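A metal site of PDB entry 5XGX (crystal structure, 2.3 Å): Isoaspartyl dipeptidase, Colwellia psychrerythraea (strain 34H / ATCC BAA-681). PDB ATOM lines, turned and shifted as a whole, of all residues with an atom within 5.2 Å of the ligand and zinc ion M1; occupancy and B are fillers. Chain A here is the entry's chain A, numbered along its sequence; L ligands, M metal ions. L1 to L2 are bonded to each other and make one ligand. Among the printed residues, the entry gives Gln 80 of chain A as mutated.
An oxygen (O3) of LIG L1 lies within hydrogen-bond range of the backbone NH of Thr 109 (3.4 Å). NH1 of Arg 237 lies within salt-bridge range of O1 of LG2 L2, 3.4 Å away. OG1 of Thr 109 lies within hydrogen-bond range of N1 of LIG L1, 2.7 Å away. O1 of LIG L1 is in hydrogen-bond range of N of Cys 297, 3.2 Å away. The guanidinium group of Arg 173 lies within salt-bridge range of an oxygen (O2) of LG2 L2. A nitrogen (N1) of LIG L1 sits close to the side-chain amide nitrogen (NE2) of Gln 80 (2.9 Å). OH of Tyr 140 sits at hydrogen-bond distance from O2 of LG2 L2. The side-chain amide nitrogen (NE2) of Gln 266 sits close to a nitrogen (N2) of LG2 L2, at 3.1 Å. The backbone NH (N) of Gly 78 sits at hydrogen-bond distance from an oxygen (O1) of LIG L1, 2.9 Å away. The backbone carbonyl oxygen of Cys 297 sits at hydrogen-bond distance from a nitrogen (N1) of LG2 L2, 2.9 Å away. The side-chain sulfur of Cys 297 is in hydrogen-bond range of an oxygen (O1) of LIG L1 (3.5 Å).
The side-chain carboxylate (OE2) of Glu 166 binds zinc ion M1 (1.8 Å). ND1 of His 205 binds zinc ion M1 (2.0 Å). NE2 of His 234 binds zinc ion M1 (2.1 Å). Zinc ion M1 is bound by O2 of LIG L1 (2.2 Å).
Tyr 140 touches zinc ion M1. Within 4 Å of zinc ion M1: Tyr 140, Glu 166, His 205 and His 234.
The backbone NH (N) of Tyr 140 sits close to the backbone carbonyl oxygen (O) of Gly 108 (3.4 Å). The side-chain hydroxyl of Tyr 140 lies close to a ring nitrogen (NE2) of His 205. The side-chain sulfur of Cys 297 lies within hydrogen-bond range of the side-chain amide nitrogen of Gln 80. N of Asp 293 lies within hydrogen-bond range of O of His 71 (3.0 Å). The side-chain carboxylate (OD2) of Asp 171 is in salt-bridge range of the guanidinium group (NH2) of Arg 173. The side-chain hydroxyl of Thr 109 lies close to the side-chain hydroxyl of Tyr 140 (3.3 Å). OG1 of Thr 109 sits close to NE2 of Gln 80 (3.5 Å). The backbone carbonyl oxygen (O) of Gly 295 lies within hydrogen-bond range of the backbone NH (N) of Gly 77.
NE2 of His 73 touches C3 of LIG L1, at 3.6 Å. Gly 77 touches the ligand. CA of Gly 108 touches O3 of LIG L1, at 3.8 Å. CE1 of Phe 260 touches C4 of LG2 L2 (3.5 Å). OD2 of Asp 293 touches C3 of LG2 L2, at 3.6 Å. CA of Gly 296 touches O1 of LIG L1, 3.7 Å away. Leu 298 touches the ligand. Pro 299 touches the ligand. Hydrophobic or aromatic side chains that line the ligand: His 73, Tyr 140, His 205, His 234, Phe 260, Leu 298 and Pro 299. Of the 26 residues printed, 19 come within 4 Å of the ligand.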
ATOM      1  N   HIS A  71      20.313  25.625   1.766  1.00  0.00           N
ATOM      2  CA  HIS A  71      20.528  25.079   0.430  1.00  0.00           C
ATOM      3  C   HIS A  71      19.506  25.605  -0.570  1.00  0.00           C
ATOM      4  O   HIS A  71      18.499  24.972  -0.813  1.00  0.00           O
ATOM      5  CB  HIS A  71      20.472  23.580   0.541  1.00  0.00           C
ATOM      6  CG  HIS A  71      21.018  22.855  -0.644  1.00  0.00           C
ATOM      7  ND1 HIS A  71      22.098  22.017  -0.566  1.00  0.00           N
ATOM      8  CD2 HIS A  71      20.582  22.777  -1.926  1.00  0.00           C
ATOM      9  CE1 HIS A  71      22.329  21.464  -1.758  1.00  0.00           C
ATOM     10  NE2 HIS A  71      21.436  21.927  -2.594  1.00  0.00           N
ATOM     11  N   HIS A  73      19.148  27.523  -4.528  1.00  0.00           N
ATOM     12  CA  HIS A  73      19.740  28.055  -5.756  1.00  0.00           C
ATOM     13  C   HIS A  73      19.093  29.379  -6.096  1.00  0.00           C
ATOM     14  O   HIS A  73      18.137  29.441  -6.883  1.00  0.00           O
ATOM     15  CB  HIS A  73      19.546  27.079  -6.881  1.00  0.00           C
ATOM     16  CG  HIS A  73      20.279  25.804  -6.632  1.00  0.00           C
ATOM     17  ND1 HIS A  73      21.609  25.650  -6.965  1.00  0.00           N
ATOM     18  CD2 HIS A  73      19.910  24.670  -6.002  1.00  0.00           C
ATOM     19  CE1 HIS A  73      22.001  24.440  -6.615  1.00  0.00           C
ATOM     20  NE2 HIS A  73      20.980  23.827  -6.043  1.00  0.00           N
ATOM     21  N   GLY A  77      18.848  27.090 -10.487  1.00  0.00           N
ATOM     22  CA  GLY A  77      19.770  26.004 -10.832  1.00  0.00           C
ATOM     23  C   GLY A  77      19.503  25.506 -12.242  1.00  0.00           C
ATOM     24  O   GLY A  77      19.304  26.280 -13.180  1.00  0.00           O
ATOM     25  N   GLY A  78      19.453  24.184 -12.385  1.00  0.00           N
ATOM     26  CA  GLY A  78      19.171  23.565 -13.641  1.00  0.00           C
ATOM     27  C   GLY A  78      20.327  23.637 -14.584  1.00  0.00           C
ATOM     28  O   GLY A  78      21.482  23.704 -14.168  1.00  0.00           O
ATOM     29  N   GLN A  80      20.873  21.095 -16.702  1.00  0.00           N
ATOM     30  CA  GLN A  80      21.365  19.713 -16.852  1.00  0.00           C
ATOM     31  C   GLN A  80      20.666  18.906 -17.914  1.00  0.00           C
ATOM     32  O   GLN A  80      20.903  17.693 -17.998  1.00  0.00           O
ATOM     33  CB  GLN A  80      21.188  18.962 -15.572  1.00  0.00           C
ATOM     34  CG  GLN A  80      21.636  19.745 -14.389  1.00  0.00           C
ATOM     35  CD  GLN A  80      21.353  18.988 -13.153  1.00  0.00           C
ATOM     36  OE1 GLN A  80      21.581  17.772 -13.111  1.00  0.00           O
ATOM     37  NE2 GLN A  80      20.809  19.673 -12.144  1.00  0.00           N
ATOM     38  N   GLY A 108      25.149  24.681  -8.203  1.00  0.00           N
ATOM     39  CA  GLY A 108      25.190  23.236  -8.223  1.00  0.00           C
ATOM     40  C   GLY A 108      25.930  22.681  -9.413  1.00  0.00           C
ATOM     41  O   GLY A 108      27.141  22.921  -9.577  1.00  0.00           O
ATOM     42  N   THR A 109      25.219  21.886 -10.207  1.00  0.00           N
ATOM     43  CA  THR A 109      25.815  21.169 -11.321  1.00  0.00           C
ATOM     44  C   THR A 109      26.402  22.139 -12.321  1.00  0.00           C
ATOM     45  O   THR A 109      27.490  21.935 -12.806  1.00  0.00           O
ATOM     46  CB  THR A 109      24.815  20.267 -12.062  1.00  0.00           C
ATOM     47  OG1 THR A 109      24.110  19.410 -11.128  1.00  0.00           O
ATOM     48  CG2 THR A 109      25.557  19.361 -13.053  1.00  0.00           C
ATOM     49  N   ASP A 110      25.648  23.188 -12.674  1.00  0.00           N
ATOM     50  CA  ASP A 110      26.119  24.162 -13.640  1.00  0.00           C
ATOM     51  C   ASP A 110      26.847  25.260 -12.873  1.00  0.00           C
ATOM     52  O   ASP A 110      26.263  26.268 -12.476  1.00  0.00           O
ATOM     53  CB  ASP A 110      24.993  24.713 -14.529  1.00  0.00           C
ATOM     54  CG  ASP A 110      25.475  25.739 -15.554  1.00  0.00           C
ATOM     55  OD1 ASP A 110      26.711  25.861 -15.768  1.00  0.00           O
ATOM     56  OD2 ASP A 110      24.590  26.435 -16.139  1.00  0.00           O
ATOM     57  N   TYR A 140      29.789  22.298  -7.519  1.00  0.00           N
ATOM     58  CA  TYR A 140      29.966  20.826  -7.603  1.00  0.00           C
ATOM     59  C   TYR A 140      31.390  20.441  -7.837  1.00  0.00           C
ATOM     60  O   TYR A 140      31.801  19.349  -7.385  1.00  0.00           O
ATOM     61  CB  TYR A 140      29.229  20.162  -8.791  1.00  0.00           C
ATOM     62  CG  TYR A 140      27.860  19.520  -8.583  1.00  0.00           C
ATOM     63  CD1 TYR A 140      26.924  20.081  -7.751  1.00  0.00           C
ATOM     64  CD2 TYR A 140      27.476  18.389  -9.296  1.00  0.00           C
ATOM     65  CE1 TYR A 140      25.639  19.528  -7.616  1.00  0.00           C
ATOM     66  CE2 TYR A 140      26.213  17.791  -9.138  1.00  0.00           C
ATOM     67  CZ  TYR A 140      25.283  18.384  -8.332  1.00  0.00           C
ATOM     68  OH  TYR A 140      23.983  17.874  -8.198  1.00  0.00           O
ATOM     69  N   GLU A 166      27.737  23.234  -2.347  1.00  0.00           N
ATOM     70  CA  GLU A 166      27.377  22.030  -2.971  1.00  0.00           C
ATOM     71  C   GLU A 166      28.478  21.346  -3.759  1.00  0.00           C
ATOM     72  O   GLU A 166      28.351  21.156  -4.966  1.00  0.00           O
ATOM     73  CB  GLU A 166      26.039  22.231  -3.608  1.00  0.00           C
ATOM     74  CG  GLU A 166      25.668  21.233  -4.604  1.00  0.00           C
ATOM     75  CD  GLU A 166      24.245  20.966  -4.565  1.00  0.00           C
ATOM     76  OE1 GLU A 166      23.538  21.873  -4.998  1.00  0.00           O
ATOM     77  OE2 GLU A 166      23.867  19.845  -4.140  1.00  0.00           O
ATOM     78  N   ASP A 171      28.675  10.783  -7.086  1.00  0.00           N
ATOM     79  CA  ASP A 171      27.694  11.232  -8.091  1.00  0.00           C
ATOM     80  C   ASP A 171      28.326  11.191  -9.479  1.00  0.00           C
ATOM     81  O   ASP A 171      29.507  11.593  -9.667  1.00  0.00           O
ATOM     82  CB  ASP A 171      27.260  12.641  -7.768  1.00  0.00           C
ATOM     83  CG  ASP A 171      25.998  13.080  -8.537  1.00  0.00           C
ATOM     84  OD1 ASP A 171      26.126  13.269  -9.763  1.00  0.00           O
ATOM     85  OD2 ASP A 171      24.886  13.229  -7.921  1.00  0.00           O
ATOM     86  N   ARG A 173      27.843  13.153 -11.823  1.00  0.00           N
ATOM     87  CA  ARG A 173      28.211  14.527 -12.236  1.00  0.00           C
ATOM     88  C   ARG A 173      29.342  15.169 -11.441  1.00  0.00           C
ATOM     89  O   ARG A 173      29.641  16.359 -11.645  1.00  0.00           O
ATOM     90  CB  ARG A 173      27.054  15.438 -12.163  1.00  0.00           C
ATOM     91  CG  ARG A 173      25.945  15.041 -13.099  1.00  0.00           C
ATOM     92  CD  ARG A 173      24.812  14.505 -12.310  1.00  0.00           C
ATOM     93  NE  ARG A 173      23.844  15.480 -11.894  1.00  0.00           N
ATOM     94  CZ  ARG A 173      23.078  15.408 -10.812  1.00  0.00           C
ATOM     95  NH1 ARG A 173      22.160  16.350 -10.634  1.00  0.00           N
ATOM     96  NH2 ARG A 173      23.242  14.454  -9.891  1.00  0.00           N
ATOM     97  N   HIS A 205      27.292  17.856  -1.741  1.00  0.00           N
ATOM     98  CA  HIS A 205      26.220  17.195  -2.502  1.00  0.00           C
ATOM     99  C   HIS A 205      26.538  15.712  -2.558  1.00  0.00           C
ATOM    100  O   HIS A 205      27.621  15.331  -2.947  1.00  0.00           O
ATOM    101  CB  HIS A 205      26.099  17.740  -3.921  1.00  0.00           C
ATOM    102  CG  HIS A 205      25.357  16.840  -4.866  1.00  0.00           C
ATOM    103  ND1 HIS A 205      24.023  17.019  -5.159  1.00  0.00           N
ATOM    104  CD2 HIS A 205      25.757  15.757  -5.580  1.00  0.00           C
ATOM    105  CE1 HIS A 205      23.633  16.087  -6.018  1.00  0.00           C
ATOM    106  NE2 HIS A 205      24.668  15.317  -6.302  1.00  0.00           N
ATOM    107  N   THR A 233      24.542  16.675   2.418  1.00  0.00           N
ATOM    108  CA  THR A 233      23.144  16.937   2.166  1.00  0.00           C
ATOM    109  C   THR A 233      22.588  15.872   1.244  1.00  0.00           C
ATOM    110  O   THR A 233      23.352  15.074   0.729  1.00  0.00           O
ATOM    111  CB  THR A 233      22.953  18.343   1.586  1.00  0.00           C
ATOM    112  OG1 THR A 233      21.573  18.734   1.703  1.00  0.00           O
ATOM    113  CG2 THR A 233      23.410  18.420   0.114  1.00  0.00           C
ATOM    114  N   HIS A 234      21.246  15.859   1.087  1.00  0.00           N
ATOM    115  CA  HIS A 234      20.479  14.889   0.314  1.00  0.00           C
ATOM    116  C   HIS A 234      20.564  13.513   0.914  1.00  0.00           C
ATOM    117  O   HIS A 234      20.417  12.499   0.227  1.00  0.00           O
ATOM    118  CB  HIS A 234      20.919  14.796  -1.152  1.00  0.00           C
ATOM    119  CG  HIS A 234      21.079  16.096  -1.853  1.00  0.00           C
ATOM    120  ND1 HIS A 234      20.182  17.126  -1.751  1.00  0.00           N
ATOM    121  CD2 HIS A 234      22.001  16.508  -2.762  1.00  0.00           C
ATOM    122  CE1 HIS A 234      20.567  18.135  -2.503  1.00  0.00           C
ATOM    123  NE2 HIS A 234      21.678  17.791  -3.118  1.00  0.00           N
ATOM    124  N   ARG A 237      18.260  10.730   0.124  1.00  0.00           N
ATOM    125  CA  ARG A 237      17.960  10.459  -1.312  1.00  0.00           C
ATOM    126  C   ARG A 237      17.869   9.000  -1.712  1.00  0.00           C
ATOM    127  O   ARG A 237      17.189   8.664  -2.702  1.00  0.00           O
ATOM    128  CB  ARG A 237      18.994  11.153  -2.269  1.00  0.00           C
ATOM    129  CG  ARG A 237      20.395  10.588  -2.232  1.00  0.00           C
ATOM    130  CD  ARG A 237      21.369  11.340  -3.127  1.00  0.00           C
ATOM    131  NE  ARG A 237      20.929  11.169  -4.505  1.00  0.00           N
ATOM    132  CZ  ARG A 237      20.766  12.129  -5.384  1.00  0.00           C
ATOM    133  NH1 ARG A 237      21.100  13.380  -5.119  1.00  0.00           N
ATOM    134  NH2 ARG A 237      20.343  11.810  -6.594  1.00  0.00           N
ATOM    135  N   THR A 258      16.961  16.716   2.464  1.00  0.00           N
ATOM    136  CA  THR A 258      16.324  17.541   1.459  1.00  0.00           C
ATOM    137  C   THR A 258      14.811  17.300   1.537  1.00  0.00           C
ATOM    138  O   THR A 258      14.343  16.154   1.473  1.00  0.00           O
ATOM    139  CB  THR A 258      16.906  17.212   0.080  1.00  0.00           C
ATOM    140  OG1 THR A 258      18.310  17.469   0.096  1.00  0.00           O
ATOM    141  CG2 THR A 258      16.271  18.080  -0.977  1.00  0.00           C
ATOM    142  N   PHE A 260      12.146  17.032  -0.321  1.00  0.00           N
ATOM    143  CA  PHE A 260      11.646  16.722  -1.670  1.00  0.00           C
ATOM    144  C   PHE A 260      10.166  17.001  -1.723  1.00  0.00           C
ATOM    145  O   PHE A 260       9.444  16.682  -0.767  1.00  0.00           O
ATOM    146  CB  PHE A 260      11.849  15.238  -2.048  1.00  0.00           C
ATOM    147  CG  PHE A 260      13.280  14.817  -2.079  1.00  0.00           C
ATOM    148  CD1 PHE A 260      14.138  15.361  -3.011  1.00  0.00           C
ATOM    149  CD2 PHE A 260      13.782  13.897  -1.152  1.00  0.00           C
ATOM    150  CE1 PHE A 260      15.476  15.020  -3.034  1.00  0.00           C
ATOM    151  CE2 PHE A 260      15.129  13.545  -1.174  1.00  0.00           C
ATOM    152  CZ  PHE A 260      15.972  14.101  -2.129  1.00  0.00           C
ATOM    153  N   THR A 264       7.819  12.397  -4.328  1.00  0.00           N
ATOM    154  CA  THR A 264       8.951  12.424  -5.303  1.00  0.00           C
ATOM    155  C   THR A 264      10.331  11.906  -4.728  1.00  0.00           C
ATOM    156  O   THR A 264      11.356  11.806  -5.461  1.00  0.00           O
ATOM    157  CB  THR A 264       9.104  13.852  -5.930  1.00  0.00           C
ATOM    158  OG1 THR A 264       9.815  14.721  -5.009  1.00  0.00           O
ATOM    159  CG2 THR A 264       7.686  14.474  -6.333  1.00  0.00           C
ATOM    160  N   GLN A 266      11.705   9.286  -4.353  1.00  0.00           N
ATOM    161  CA  GLN A 266      12.608   8.712  -5.349  1.00  0.00           C
ATOM    162  C   GLN A 266      12.558   7.299  -4.815  1.00  0.00           C
ATOM    163  O   GLN A 266      11.435   6.887  -4.439  1.00  0.00           O
ATOM    164  CB  GLN A 266      13.976   9.491  -5.299  1.00  0.00           C
ATOM    165  CG  GLN A 266      14.737   9.763  -6.607  1.00  0.00           C
ATOM    166  CD  GLN A 266      16.092  10.456  -6.371  1.00  0.00           C
ATOM    167  OE1 GLN A 266      16.451  10.805  -5.221  1.00  0.00           O
ATOM    168  NE2 GLN A 266      16.847  10.662  -7.471  1.00  0.00           N
ATOM    169  N   ASP A 293      16.305  22.972  -1.192  1.00  0.00           N
ATOM    170  CA  ASP A 293      16.807  22.919  -2.558  1.00  0.00           C
ATOM    171  C   ASP A 293      16.024  23.827  -3.518  1.00  0.00           C
ATOM    172  O   ASP A 293      15.891  23.519  -4.698  1.00  0.00           O
ATOM    173  CB  ASP A 293      16.830  21.468  -3.041  1.00  0.00           C
ATOM    174  CG  ASP A 293      17.883  21.212  -4.078  1.00  0.00           C
ATOM    175  OD1 ASP A 293      18.570  22.174  -4.488  1.00  0.00           O
ATOM    176  OD2 ASP A 293      18.035  20.028  -4.462  1.00  0.00           O
ATOM    177  N   GLY A 295      14.808  26.448  -6.164  1.00  0.00           N
ATOM    178  CA  GLY A 295      15.380  26.810  -7.439  1.00  0.00           C
ATOM    179  C   GLY A 295      16.185  25.716  -8.149  1.00  0.00           C
ATOM    180  O   GLY A 295      16.609  25.930  -9.286  1.00  0.00           O
ATOM    181  N   GLY A 296      16.389  24.571  -7.511  1.00  0.00           N
ATOM    182  CA  GLY A 296      17.124  23.460  -8.080  1.00  0.00           C
ATOM    183  C   GLY A 296      16.195  22.665  -8.954  1.00  0.00           C
ATOM    184  O   GLY A 296      14.984  22.771  -8.818  1.00  0.00           O
ATOM    185  N   CYS A 297      16.762  21.914  -9.888  1.00  0.00           N
ATOM    186  CA  CYS A 297      16.036  20.847 -10.579  1.00  0.00           C
ATOM    187  C   CYS A 297      16.369  19.532  -9.854  1.00  0.00           C
ATOM    188  O   CYS A 297      17.481  19.367  -9.342  1.00  0.00           O
ATOM    189  CB  CYS A 297      16.413  20.781 -12.058  1.00  0.00           C
ATOM    190  SG  CYS A 297      18.058  20.101 -12.352  1.00  0.00           S
ATOM    191  N   LEU A 298      15.396  18.628  -9.806  1.00  0.00           N
ATOM    192  CA  LEU A 298      15.517  17.300  -9.169  1.00  0.00           C
ATOM    193  C   LEU A 298      15.380  16.215 -10.268  1.00  0.00           C
ATOM    194  O   LEU A 298      14.267  15.828 -10.623  1.00  0.00           O
ATOM    195  CB  LEU A 298      14.432  17.146  -8.079  1.00  0.00           C
ATOM    196  CG  LEU A 298      14.278  18.282  -7.046  1.00  0.00           C
ATOM    197  CD1 LEU A 298      13.220  17.924  -6.005  1.00  0.00           C
ATOM    198  CD2 LEU A 298      15.588  18.669  -6.370  1.00  0.00           C
ATOM    199  N   PRO A 299      16.526  15.761 -10.860  1.00  0.00           N
ATOM    200  CA  PRO A 299      16.477  14.879 -12.068  1.00  0.00           C
ATOM    201  C   PRO A 299      16.110  13.374 -11.871  1.00  0.00           C
ATOM    202  O   PRO A 299      16.505  12.739 -10.881  1.00  0.00           O
ATOM    203  CB  PRO A 299      17.885  15.053 -12.681  1.00  0.00           C
ATOM    204  CG  PRO A 299      18.767  15.476 -11.552  1.00  0.00           C
ATOM    205  CD  PRO A 299      17.901  16.236 -10.576  1.00  0.00           C
HETATM  206  N1  LIG L   1      22.021  19.903  -9.500  1.00  0.00           N
HETATM  207  C1  LIG L   1      21.579  21.128  -8.808  1.00  0.00           C
HETATM  208  C2  LIG L   1      21.125  22.222  -9.866  1.00  0.00           C
HETATM  209  O1  LIG L   1      19.924  22.278 -10.273  1.00  0.00           O
HETATM  210  C3  LIG L   1      20.442  20.776  -7.835  1.00  0.00           C
HETATM  211  C4  LIG L   1      20.620  19.416  -7.247  1.00  0.00           C
HETATM  212  O2  LIG L   1      21.643  19.069  -6.600  1.00  0.00           O
HETATM  213  O3  LIG L   1      21.986  23.023 -10.219  1.00  0.00           O
HETATM  214  N1  LG2 L   2      19.531  18.587  -7.520  1.00  0.00           N
HETATM  215  C1  LG2 L   2      19.352  17.179  -7.162  1.00  0.00           C
HETATM  216  C2  LG2 L   2      20.439  16.307  -7.880  1.00  0.00           C
HETATM  217  O1  LG2 L   2      20.282  15.055  -7.906  1.00  0.00           O
HETATM  218  C3  LG2 L   2      19.406  16.900  -5.595  1.00  0.00           C
HETATM  219  C4  LG2 L   2      18.133  16.142  -5.010  1.00  0.00           C
HETATM  220  C5  LG2 L   2      17.859  14.679  -5.633  1.00  0.00           C
HETATM  221  C6  LG2 L   2      16.920  14.700  -6.892  1.00  0.00           C
HETATM  222  N2  LG2 L   2      15.957  13.592  -6.842  1.00  0.00           N
HETATM  223  O2  LG2 L   2      21.373  16.942  -8.401  1.00  0.00           O
HETATM  224 ZN    ZN M   1      22.746  18.564  -4.780  1.00  0.00          ZN
HETATM  225 ZN    ZN M   2      20.991  21.236  -4.847  1.00  0.00          ZN
